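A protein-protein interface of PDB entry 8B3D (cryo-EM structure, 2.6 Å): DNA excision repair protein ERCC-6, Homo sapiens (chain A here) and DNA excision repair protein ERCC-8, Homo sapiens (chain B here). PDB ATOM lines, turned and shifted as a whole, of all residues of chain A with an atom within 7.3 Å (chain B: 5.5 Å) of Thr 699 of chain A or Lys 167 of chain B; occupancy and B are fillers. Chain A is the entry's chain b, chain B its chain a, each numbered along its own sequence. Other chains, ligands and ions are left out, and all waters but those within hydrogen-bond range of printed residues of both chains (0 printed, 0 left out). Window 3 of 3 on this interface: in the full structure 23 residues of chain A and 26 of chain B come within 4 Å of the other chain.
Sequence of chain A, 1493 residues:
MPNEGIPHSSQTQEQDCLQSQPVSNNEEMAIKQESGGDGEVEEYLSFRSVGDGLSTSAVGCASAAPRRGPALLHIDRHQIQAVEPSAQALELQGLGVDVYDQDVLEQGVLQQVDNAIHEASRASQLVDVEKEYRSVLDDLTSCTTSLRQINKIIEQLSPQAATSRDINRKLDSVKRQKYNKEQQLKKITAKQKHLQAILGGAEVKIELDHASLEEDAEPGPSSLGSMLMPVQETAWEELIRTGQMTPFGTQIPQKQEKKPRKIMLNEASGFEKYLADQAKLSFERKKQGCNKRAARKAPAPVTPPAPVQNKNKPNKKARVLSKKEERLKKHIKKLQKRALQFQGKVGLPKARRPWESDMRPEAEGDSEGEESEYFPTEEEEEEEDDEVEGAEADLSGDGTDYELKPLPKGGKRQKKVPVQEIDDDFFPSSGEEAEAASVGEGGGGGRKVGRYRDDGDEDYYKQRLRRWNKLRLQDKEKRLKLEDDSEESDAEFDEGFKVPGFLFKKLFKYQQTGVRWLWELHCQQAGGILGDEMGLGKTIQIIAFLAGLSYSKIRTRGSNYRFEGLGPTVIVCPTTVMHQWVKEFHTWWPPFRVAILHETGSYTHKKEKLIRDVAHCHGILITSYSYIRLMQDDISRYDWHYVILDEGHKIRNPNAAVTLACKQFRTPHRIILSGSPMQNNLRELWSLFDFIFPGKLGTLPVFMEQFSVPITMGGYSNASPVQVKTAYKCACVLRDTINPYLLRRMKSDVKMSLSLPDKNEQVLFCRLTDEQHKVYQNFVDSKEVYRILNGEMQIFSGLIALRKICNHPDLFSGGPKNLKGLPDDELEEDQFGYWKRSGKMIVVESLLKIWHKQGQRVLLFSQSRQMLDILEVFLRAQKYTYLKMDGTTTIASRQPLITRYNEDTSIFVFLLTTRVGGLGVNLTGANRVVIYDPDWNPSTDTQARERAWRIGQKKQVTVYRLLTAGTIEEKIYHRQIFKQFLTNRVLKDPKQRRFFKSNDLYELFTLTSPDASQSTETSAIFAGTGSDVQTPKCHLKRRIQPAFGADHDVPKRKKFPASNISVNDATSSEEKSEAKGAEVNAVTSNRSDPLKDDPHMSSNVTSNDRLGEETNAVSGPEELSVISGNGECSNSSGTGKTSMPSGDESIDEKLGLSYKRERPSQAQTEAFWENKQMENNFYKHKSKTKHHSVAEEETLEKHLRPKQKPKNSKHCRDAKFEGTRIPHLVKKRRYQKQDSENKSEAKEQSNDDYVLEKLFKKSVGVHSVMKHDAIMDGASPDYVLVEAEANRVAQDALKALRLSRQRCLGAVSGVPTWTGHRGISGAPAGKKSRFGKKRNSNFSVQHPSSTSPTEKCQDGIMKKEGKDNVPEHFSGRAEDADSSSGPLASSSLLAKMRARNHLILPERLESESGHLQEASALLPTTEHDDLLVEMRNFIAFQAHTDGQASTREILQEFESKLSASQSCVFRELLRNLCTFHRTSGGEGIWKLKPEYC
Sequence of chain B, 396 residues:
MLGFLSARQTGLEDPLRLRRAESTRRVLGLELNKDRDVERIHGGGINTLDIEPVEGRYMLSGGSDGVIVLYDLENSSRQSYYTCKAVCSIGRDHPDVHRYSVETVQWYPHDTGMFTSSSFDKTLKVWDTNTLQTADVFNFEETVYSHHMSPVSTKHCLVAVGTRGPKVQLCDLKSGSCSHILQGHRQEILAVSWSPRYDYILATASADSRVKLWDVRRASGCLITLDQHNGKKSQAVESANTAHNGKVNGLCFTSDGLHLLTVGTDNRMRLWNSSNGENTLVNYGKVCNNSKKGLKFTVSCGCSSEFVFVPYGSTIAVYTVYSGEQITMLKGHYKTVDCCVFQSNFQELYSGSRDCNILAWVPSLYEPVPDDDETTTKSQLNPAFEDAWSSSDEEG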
ATOM      1  N   TRP A 686      14.210 -15.466  12.711  1.00  0.00           N
ATOM      2  CA  TRP A 686      14.140 -16.288  11.510  1.00  0.00           C
ATOM      3  C   TRP A 686      14.064 -17.766  11.856  1.00  0.00           C
ATOM      4  O   TRP A 686      13.338 -18.518  11.206  1.00  0.00           O
ATOM      5  CB  TRP A 686      15.338 -16.042  10.605  1.00  0.00           C
ATOM      6  CG  TRP A 686      15.215 -16.817   9.338  1.00  0.00           C
ATOM      7  CD1 TRP A 686      14.619 -16.407   8.187  1.00  0.00           C
ATOM      8  CD2 TRP A 686      15.670 -18.153   9.100  1.00  0.00           C
ATOM      9  NE1 TRP A 686      14.685 -17.395   7.242  1.00  0.00           N
ATOM     10  CE2 TRP A 686      15.324 -18.480   7.778  1.00  0.00           C
ATOM     11  CE3 TRP A 686      16.341 -19.101   9.876  1.00  0.00           C
ATOM     12  CZ2 TRP A 686      15.628 -19.713   7.212  1.00  0.00           C
ATOM     13  CZ3 TRP A 686      16.641 -20.322   9.314  1.00  0.00           C
ATOM     14  CH2 TRP A 686      16.287 -20.617   7.996  1.00  0.00           C
ATOM     15  N   ASP A 690      10.986 -20.007  10.801  1.00  0.00           N
ATOM     16  CA  ASP A 690      11.219 -21.193   9.999  1.00  0.00           C
ATOM     17  C   ASP A 690      10.571 -22.406  10.638  1.00  0.00           C
ATOM     18  O   ASP A 690      10.029 -23.256   9.925  1.00  0.00           O
ATOM     19  CB  ASP A 690      12.722 -21.425   9.825  1.00  0.00           C
ATOM     20  CG  ASP A 690      13.043 -22.534   8.831  1.00  0.00           C
ATOM     21  OD1 ASP A 690      12.126 -23.254   8.387  1.00  0.00           O
ATOM     22  OD2 ASP A 690      14.233 -22.700   8.501  1.00  0.00           O
ATOM     23  N   PRO A 694       7.596 -22.413   7.573  1.00  0.00           N
ATOM     24  CA  PRO A 694       8.929 -22.355   6.940  1.00  0.00           C
ATOM     25  C   PRO A 694       9.120 -21.283   5.875  1.00  0.00           C
ATOM     26  O   PRO A 694      10.258 -20.864   5.640  1.00  0.00           O
ATOM     27  CB  PRO A 694       9.069 -23.756   6.336  1.00  0.00           C
ATOM     28  CG  PRO A 694       8.301 -24.620   7.239  1.00  0.00           C
ATOM     29  CD  PRO A 694       7.131 -23.805   7.710  1.00  0.00           C
ATOM     30  N   GLY A 695       8.053 -20.824   5.230  1.00  0.00           N
ATOM     31  CA  GLY A 695       8.198 -20.003   4.045  1.00  0.00           C
ATOM     32  C   GLY A 695       8.218 -18.495   4.214  1.00  0.00           C
ATOM     33  O   GLY A 695       8.847 -17.815   3.399  1.00  0.00           O
ATOM     34  N   LYS A 696       7.559 -17.953   5.246  1.00  0.00           N
ATOM     35  CA  LYS A 696       7.248 -16.524   5.290  1.00  0.00           C
ATOM     36  C   LYS A 696       8.520 -15.696   5.216  1.00  0.00           C
ATOM     37  O   LYS A 696       8.708 -14.913   4.281  1.00  0.00           O
ATOM     38  CB  LYS A 696       6.478 -16.153   6.562  1.00  0.00           C
ATOM     39  CG  LYS A 696       5.970 -14.722   6.625  1.00  0.00           C
ATOM     40  CD  LYS A 696       4.968 -14.399   5.504  1.00  0.00           C
ATOM     41  CE  LYS A 696       3.710 -15.253   5.591  1.00  0.00           C
ATOM     42  NZ  LYS A 696       2.508 -14.557   5.066  1.00  0.00           N
ATOM     43  N   LEU A 697       9.388 -15.854   6.206  1.00  0.00           N
ATOM     44  CA  LEU A 697      10.744 -15.353   6.085  1.00  0.00           C
ATOM     45  C   LEU A 697      11.550 -16.364   5.285  1.00  0.00           C
ATOM     46  O   LEU A 697      11.598 -17.549   5.626  1.00  0.00           O
ATOM     47  CB  LEU A 697      11.352 -15.126   7.467  1.00  0.00           C
ATOM     48  CG  LEU A 697      10.402 -14.513   8.502  1.00  0.00           C
ATOM     49  CD1 LEU A 697      11.094 -14.319   9.832  1.00  0.00           C
ATOM     50  CD2 LEU A 697       9.843 -13.195   7.995  1.00  0.00           C
ATOM     51  N   GLY A 698      12.168 -15.900   4.204  1.00  0.00           N
ATOM     52  CA  GLY A 698      12.714 -16.807   3.215  1.00  0.00           C
ATOM     53  C   GLY A 698      13.915 -17.587   3.703  1.00  0.00           C
ATOM     54  O   GLY A 698      14.053 -17.840   4.901  1.00  0.00           O
ATOM     55  N   THR A 699      14.782 -17.995   2.786  1.00  0.00           N
ATOM     56  CA  THR A 699      16.017 -18.642   3.194  1.00  0.00           C
ATOM     57  C   THR A 699      16.838 -17.679   4.040  1.00  0.00           C
ATOM     58  O   THR A 699      16.757 -16.458   3.881  1.00  0.00           O
ATOM     59  CB  THR A 699      16.815 -19.092   1.973  1.00  0.00           C
ATOM     60  OG1 THR A 699      17.103 -17.958   1.146  1.00  0.00           O
ATOM     61  CG2 THR A 699      16.028 -20.118   1.171  1.00  0.00           C
ATOM     62  N   LEU A 700      17.613 -18.240   4.966  1.00  0.00           N
ATOM     63  CA  LEU A 700      18.329 -17.439   5.951  1.00  0.00           C
ATOM     64  C   LEU A 700      19.229 -16.390   5.300  1.00  0.00           C
ATOM     65  O   LEU A 700      19.249 -15.250   5.772  1.00  0.00           O
ATOM     66  CB  LEU A 700      19.135 -18.342   6.891  1.00  0.00           C
ATOM     67  CG  LEU A 700      19.877 -17.690   8.065  1.00  0.00           C
ATOM     68  CD1 LEU A 700      19.067 -16.608   8.766  1.00  0.00           C
ATOM     69  CD2 LEU A 700      20.295 -18.759   9.058  1.00  0.00           C
ATOM     70  N   PRO A 701      19.986 -16.708   4.232  1.00  0.00           N
ATOM     71  CA  PRO A 701      20.726 -15.644   3.532  1.00  0.00           C
ATOM     72  C   PRO A 701      19.845 -14.480   3.100  1.00  0.00           C
ATOM     73  O   PRO A 701      20.197 -13.309   3.292  1.00  0.00           O
ATOM     74  CB  PRO A 701      21.302 -16.366   2.310  1.00  0.00           C
ATOM     75  CG  PRO A 701      21.427 -17.774   2.712  1.00  0.00           C
ATOM     76  CD  PRO A 701      20.463 -18.046   3.832  1.00  0.00           C
ATOM     77  N   VAL A 702      18.693 -14.804   2.511  1.00  0.00           N
ATOM     78  CA  VAL A 702      17.788 -13.766   2.030  1.00  0.00           C
ATOM     79  C   VAL A 702      17.261 -12.942   3.194  1.00  0.00           C
ATOM     80  O   VAL A 702      17.189 -11.710   3.115  1.00  0.00           O
ATOM     81  CB  VAL A 702      16.644 -14.391   1.211  1.00  0.00           C
ATOM     82  CG1 VAL A 702      15.637 -13.328   0.798  1.00  0.00           C
ATOM     83  CG2 VAL A 702      17.193 -15.095  -0.019  1.00  0.00           C
ATOM     84  N   PHE A 703      16.874 -13.601   4.288  1.00  0.00           N
ATOM     85  CA  PHE A 703      16.377 -12.863   5.443  1.00  0.00           C
ATOM     86  C   PHE A 703      17.454 -11.947   5.999  1.00  0.00           C
ATOM     87  O   PHE A 703      17.182 -10.792   6.338  1.00  0.00           O
ATOM     88  CB  PHE A 703      15.888 -13.820   6.527  1.00  0.00           C
ATOM     89  CG  PHE A 703      15.495 -13.126   7.799  1.00  0.00           C
ATOM     90  CD1 PHE A 703      14.245 -12.552   7.930  1.00  0.00           C
ATOM     91  CD2 PHE A 703      16.380 -13.032   8.859  1.00  0.00           C
ATOM     92  CE1 PHE A 703      13.884 -11.906   9.091  1.00  0.00           C
ATOM     93  CE2 PHE A 703      16.020 -12.389  10.022  1.00  0.00           C
ATOM     94  CZ  PHE A 703      14.771 -11.827  10.138  1.00  0.00           C
ATOM     95  N   MET A 704      18.685 -12.453   6.113  1.00  0.00           N
ATOM     96  CA  MET A 704      19.795 -11.605   6.529  1.00  0.00           C
ATOM     97  C   MET A 704      19.870 -10.362   5.659  1.00  0.00           C
ATOM     98  O   MET A 704      19.662  -9.248   6.148  1.00  0.00           O
ATOM     99  CB  MET A 704      21.120 -12.372   6.465  1.00  0.00           C
ATOM    100  CG  MET A 704      21.318 -13.499   7.485  1.00  0.00           C
ATOM    101  SD  MET A 704      20.602 -13.239   9.115  1.00  0.00           S
ATOM    102  CE  MET A 704      21.995 -12.505   9.966  1.00  0.00           C
ATOM    103  N   GLU A 705      20.051 -10.554   4.350  1.00  0.00           N
ATOM    104  CA  GLU A 705      20.290  -9.430   3.451  1.00  0.00           C
ATOM    105  C   GLU A 705      19.132  -8.437   3.466  1.00  0.00           C
ATOM    106  O   GLU A 705      19.352  -7.225   3.364  1.00  0.00           O
ATOM    107  CB  GLU A 705      20.535  -9.951   2.032  1.00  0.00           C
ATOM    108  CG  GLU A 705      20.844  -8.876   0.991  1.00  0.00           C
ATOM    109  CD  GLU A 705      22.151  -8.156   1.264  1.00  0.00           C
ATOM    110  OE1 GLU A 705      23.037  -8.753   1.911  1.00  0.00           O
ATOM    111  OE2 GLU A 705      22.292  -6.994   0.830  1.00  0.00           O
ATOM    112  N   VAL B 161       5.401 -14.835  -8.150  1.00  0.00           N
ATOM    113  CA  VAL B 161       6.467 -14.621  -9.121  1.00  0.00           C
ATOM    114  C   VAL B 161       7.246 -15.916  -9.271  1.00  0.00           C
ATOM    115  O   VAL B 161       7.664 -16.516  -8.272  1.00  0.00           O
ATOM    116  CB  VAL B 161       7.405 -13.476  -8.695  1.00  0.00           C
ATOM    117  CG1 VAL B 161       8.354 -13.115  -9.824  1.00  0.00           C
ATOM    118  CG2 VAL B 161       6.605 -12.264  -8.259  1.00  0.00           C
ATOM    119  N   GLY B 162       7.435 -16.343 -10.516  1.00  0.00           N
ATOM    120  CA  GLY B 162       8.259 -17.489 -10.843  1.00  0.00           C
ATOM    121  C   GLY B 162       9.486 -17.036 -11.618  1.00  0.00           C
ATOM    122  O   GLY B 162       9.372 -16.490 -12.719  1.00  0.00           O
ATOM    123  N   THR B 163      10.646 -17.261 -11.012  1.00  0.00           N
ATOM    124  CA  THR B 163      11.949 -16.895 -11.546  1.00  0.00           C
ATOM    125  C   THR B 163      12.705 -18.170 -11.911  1.00  0.00           C
ATOM    126  O   THR B 163      12.182 -19.280 -11.789  1.00  0.00           O
ATOM    127  CB  THR B 163      12.729 -16.060 -10.527  1.00  0.00           C
ATOM    128  OG1 THR B 163      12.841 -16.787  -9.297  1.00  0.00           O
ATOM    129  CG2 THR B 163      12.038 -14.732 -10.260  1.00  0.00           C
ATOM    130  N   GLY B 165      15.089 -19.165 -10.151  1.00  0.00           N
ATOM    131  CA  GLY B 165      15.282 -19.824  -8.886  1.00  0.00           C
ATOM    132  C   GLY B 165      14.234 -20.908  -8.718  1.00  0.00           C
ATOM    133  O   GLY B 165      13.168 -20.846  -9.335  1.00  0.00           O
ATOM    134  N   PRO B 166      14.500 -21.926  -7.894  1.00  0.00           N
ATOM    135  CA  PRO B 166      13.500 -22.984  -7.704  1.00  0.00           C
ATOM    136  C   PRO B 166      12.374 -22.612  -6.754  1.00  0.00           C
ATOM    137  O   PRO B 166      11.553 -23.476  -6.433  1.00  0.00           O
ATOM    138  CB  PRO B 166      14.323 -24.152  -7.131  1.00  0.00           C
ATOM    139  CG  PRO B 166      15.682 -23.623  -6.835  1.00  0.00           C
ATOM    140  CD  PRO B 166      15.700 -22.156  -7.075  1.00  0.00           C
ATOM    141  N   LYS B 167      12.312 -21.364  -6.301  1.00  0.00           N
ATOM    142  CA  LYS B 167      11.350 -20.920  -5.308  1.00  0.00           C
ATOM    143  C   LYS B 167      10.326 -19.997  -5.956  1.00  0.00           C
ATOM    144  O   LYS B 167      10.673 -19.128  -6.759  1.00  0.00           O
ATOM    145  CB  LYS B 167      12.052 -20.177  -4.168  1.00  0.00           C
ATOM    146  CG  LYS B 167      13.161 -20.960  -3.484  1.00  0.00           C
ATOM    147  CD  LYS B 167      12.631 -22.151  -2.707  1.00  0.00           C
ATOM    148  CE  LYS B 167      13.612 -22.621  -1.636  1.00  0.00           C
ATOM    149  NZ  LYS B 167      15.038 -22.315  -1.954  1.00  0.00           N
ATOM    150  N   VAL B 168       9.060 -20.195  -5.604  1.00  0.00           N
ATOM    151  CA  VAL B 168       7.984 -19.293  -6.001  1.00  0.00           C
ATOM    152  C   VAL B 168       7.929 -18.178  -4.972  1.00  0.00           C
ATOM    153  O   VAL B 168       7.661 -18.432  -3.793  1.00  0.00           O
ATOM    154  CB  VAL B 168       6.621 -20.008  -6.080  1.00  0.00           C
ATOM    155  CG1 VAL B 168       5.611 -19.117  -6.791  1.00  0.00           C
ATOM    156  CG2 VAL B 168       6.699 -21.366  -6.776  1.00  0.00           C
ATOM    157  N   GLN B 169       8.163 -16.946  -5.407  1.00  0.00           N
ATOM    158  CA  GLN B 169       8.114 -15.795  -4.517  1.00  0.00           C
ATOM    159  C   GLN B 169       6.678 -15.303  -4.427  1.00  0.00           C
ATOM    160  O   GLN B 169       5.935 -15.379  -5.407  1.00  0.00           O
ATOM    161  CB  GLN B 169       9.029 -14.676  -5.012  1.00  0.00           C
ATOM    162  CG  GLN B 169      10.498 -15.076  -5.160  1.00  0.00           C
ATOM    163  CD  GLN B 169      11.395 -14.535  -4.058  1.00  0.00           C
ATOM    164  OE1 GLN B 169      11.075 -13.548  -3.396  1.00  0.00           O
ATOM    165  NE2 GLN B 169      12.533 -15.187  -3.860  1.00  0.00           N
ATOM    166  N   SER B 179       9.581 -11.638   1.092  1.00  0.00           N
ATOM    167  CA  SER B 179      10.327 -12.710   1.737  1.00  0.00           C
ATOM    168  C   SER B 179       9.650 -14.069   1.599  1.00  0.00           C
ATOM    169  O   SER B 179      10.333 -15.097   1.564  1.00  0.00           O
ATOM    170  CB  SER B 179      10.524 -12.382   3.218  1.00  0.00           C
ATOM    171  OG  SER B 179       9.282 -12.311   3.893  1.00  0.00           O
ATOM    172  N   ILE B 181       8.307 -17.400   0.366  1.00  0.00           N
ATOM    173  CA  ILE B 181       8.658 -18.284  -0.738  1.00  0.00           C
ATOM    174  C   ILE B 181       8.015 -19.645  -0.508  1.00  0.00           C
ATOM    175  O   ILE B 181       7.701 -20.010   0.629  1.00  0.00           O
ATOM    176  CB  ILE B 181      10.189 -18.410  -0.903  1.00  0.00           C
ATOM    177  CG1 ILE B 181      10.846 -18.972   0.364  1.00  0.00           C
ATOM    178  CG2 ILE B 181      10.791 -17.064  -1.266  1.00  0.00           C
ATOM    179  CD1 ILE B 181      12.299 -19.336   0.178  1.00  0.00           C
ATOM    180  N   LEU B 182       7.813 -20.387  -1.594  1.00  0.00           N
ATOM    181  CA  LEU B 182       7.289 -21.747  -1.545  1.00  0.00           C
ATOM    182  C   LEU B 182       8.352 -22.715  -2.047  1.00  0.00           C
ATOM    183  O   LEU B 182       8.891 -22.535  -3.143  1.00  0.00           O
ATOM    184  CB  LEU B 182       6.020 -21.877  -2.390  1.00  0.00           C
ATOM    185  CG  LEU B 182       4.885 -20.895  -2.093  1.00  0.00           C
ATOM    186  CD1 LEU B 182       3.935 -20.811  -3.270  1.00  0.00           C
ATOM    187  CD2 LEU B 182       4.141 -21.308  -0.840  1.00  0.00           C
ATOM    188  N   GLN B 183       8.643 -23.740  -1.250  1.00  0.00           N
ATOM    189  CA  GLN B 183       9.655 -24.736  -1.575  1.00  0.00           C
ATOM    190  C   GLN B 183       8.984 -25.995  -2.099  1.00  0.00           C
ATOM    191  O   GLN B 183       7.899 -26.364  -1.641  1.00  0.00           O
ATOM    192  CB  GLN B 183      10.504 -25.104  -0.353  1.00  0.00           C
ATOM    193  CG  GLN B 183      11.130 -23.927   0.386  1.00  0.00           C
ATOM    194  CD  GLN B 183      10.296 -23.439   1.562  1.00  0.00           C
ATOM    195  OE1 GLN B 183       9.311 -24.066   1.953  1.00  0.00           O
ATOM    196  NE2 GLN B 183      10.703 -22.319   2.145  1.00  0.00           N
ATOM    197  N   GLY B 184       9.652 -26.672  -3.028  1.00  0.00           N
ATOM    198  CA  GLY B 184       9.163 -27.936  -3.542  1.00  0.00           C
ATOM    199  C   GLY B 184       9.469 -28.175  -5.005  1.00  0.00           C
ATOM    200  O   GLY B 184       9.495 -29.326  -5.448  1.00  0.00           O
ATOM    201  N   ILE B 189      10.843 -21.926 -12.534  1.00  0.00           N
ATOM    202  CA  ILE B 189       9.389 -21.921 -12.459  1.00  0.00           C
ATOM    203  C   ILE B 189       8.880 -21.085 -13.623  1.00  0.00           C
ATOM    204  O   ILE B 189       8.835 -19.857 -13.544  1.00  0.00           O
ATOM    205  CB  ILE B 189       8.901 -21.370 -11.117  1.00  0.00           C
ATOM    206  CG1 ILE B 189       9.366 -22.282  -9.981  1.00  0.00           C
ATOM    207  CG2 ILE B 189       7.389 -21.248 -11.121  1.00  0.00           C
ATOM    208  CD1 ILE B 189       9.376 -21.615  -8.647  1.00  0.00           C
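Among the printed residues, merely in contact across the chains: Pro 694 of chain A with Gln 183 of chain B (3.8 Å), Gly 695 of chain A with Ser 179 of chain B (3.6 Å), Gly 695 of chain A with Gln 183 of chain B (3.9 Å), Gly 698 of chain A with Ile 181 of chain B (3.97 Å), Thr 699 of chain A with Lys 167 of chain B (3.9 Å) and Thr 699 of chain A with Ile 181 of chain B (3.8 Å).
Of the 14 printed residues of chain A, 5 touch a printed residue of chain B. Printed residues of chain A that touch a printed residue of chain B: Pro 694, Gly 695, Lys 696, Gly 698 and Thr 699. Among the printed residues, no Asp or Glu carboxylate lies within 4 Å of a Lys or Arg side-chain nitrogen of the other chain.
The backbone NH of Ile 181 of chain B is in hydrogen-bond range of the backbone carbonyl oxygen of Gly 695 of chain A, 3.1 Å away. O of Lys 696 of chain A lies within hydrogen-bond range of OG of Ser 179 of chain B (2.7 Å). The backbone carbonyl oxygen of Ser 179 of chain B lies within hydrogen-bond range of the backbone NH of Gly 698 of chain A, 3.3 Å away.
Of the printed residues of chain B, Pro 694 of chain A touches Gln 183 (3.8 Å). Of the printed residues of chain B, Lys 696 of chain A touches Ser 179. Leu 697 of chain A touches none of the printed residues of chain B. Thr 699 of chain A touches just these residues of chain B: Lys 167 (3.9 Å) and Ile 181 (3.8 Å). Of chain A, only Thr 699 comes within 4 Å of Lys 167 of chain B. Of the printed residues of chain A, Ser 179 of chain B touches Gly 695, Lys 696 and Gly 698. Printed residues of chain A within 4 Å of Ile 181 of chain B: Gly 695 (3.1 Å), Gly 698 (3.97 Å) and Thr 699 (3.8 Å). Of the printed residues of chain A, Gln 183 of chain B touches Pro 694 (3.8 Å) and Gly 695 (3.9 Å). The nearest printed residue of chain A that does not touch Lys 167 of chain B is Gly 698 of chain A (7.3 Å). The nearest printed residue of chain A that does not touch Ile 181 of chain B is Lys 696 of chain A (4.7 Å).
NE1 of Trp 686 of chain A sits at hydrogen-bond distance from O of Gly 698 of chain A (2.5 Å).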
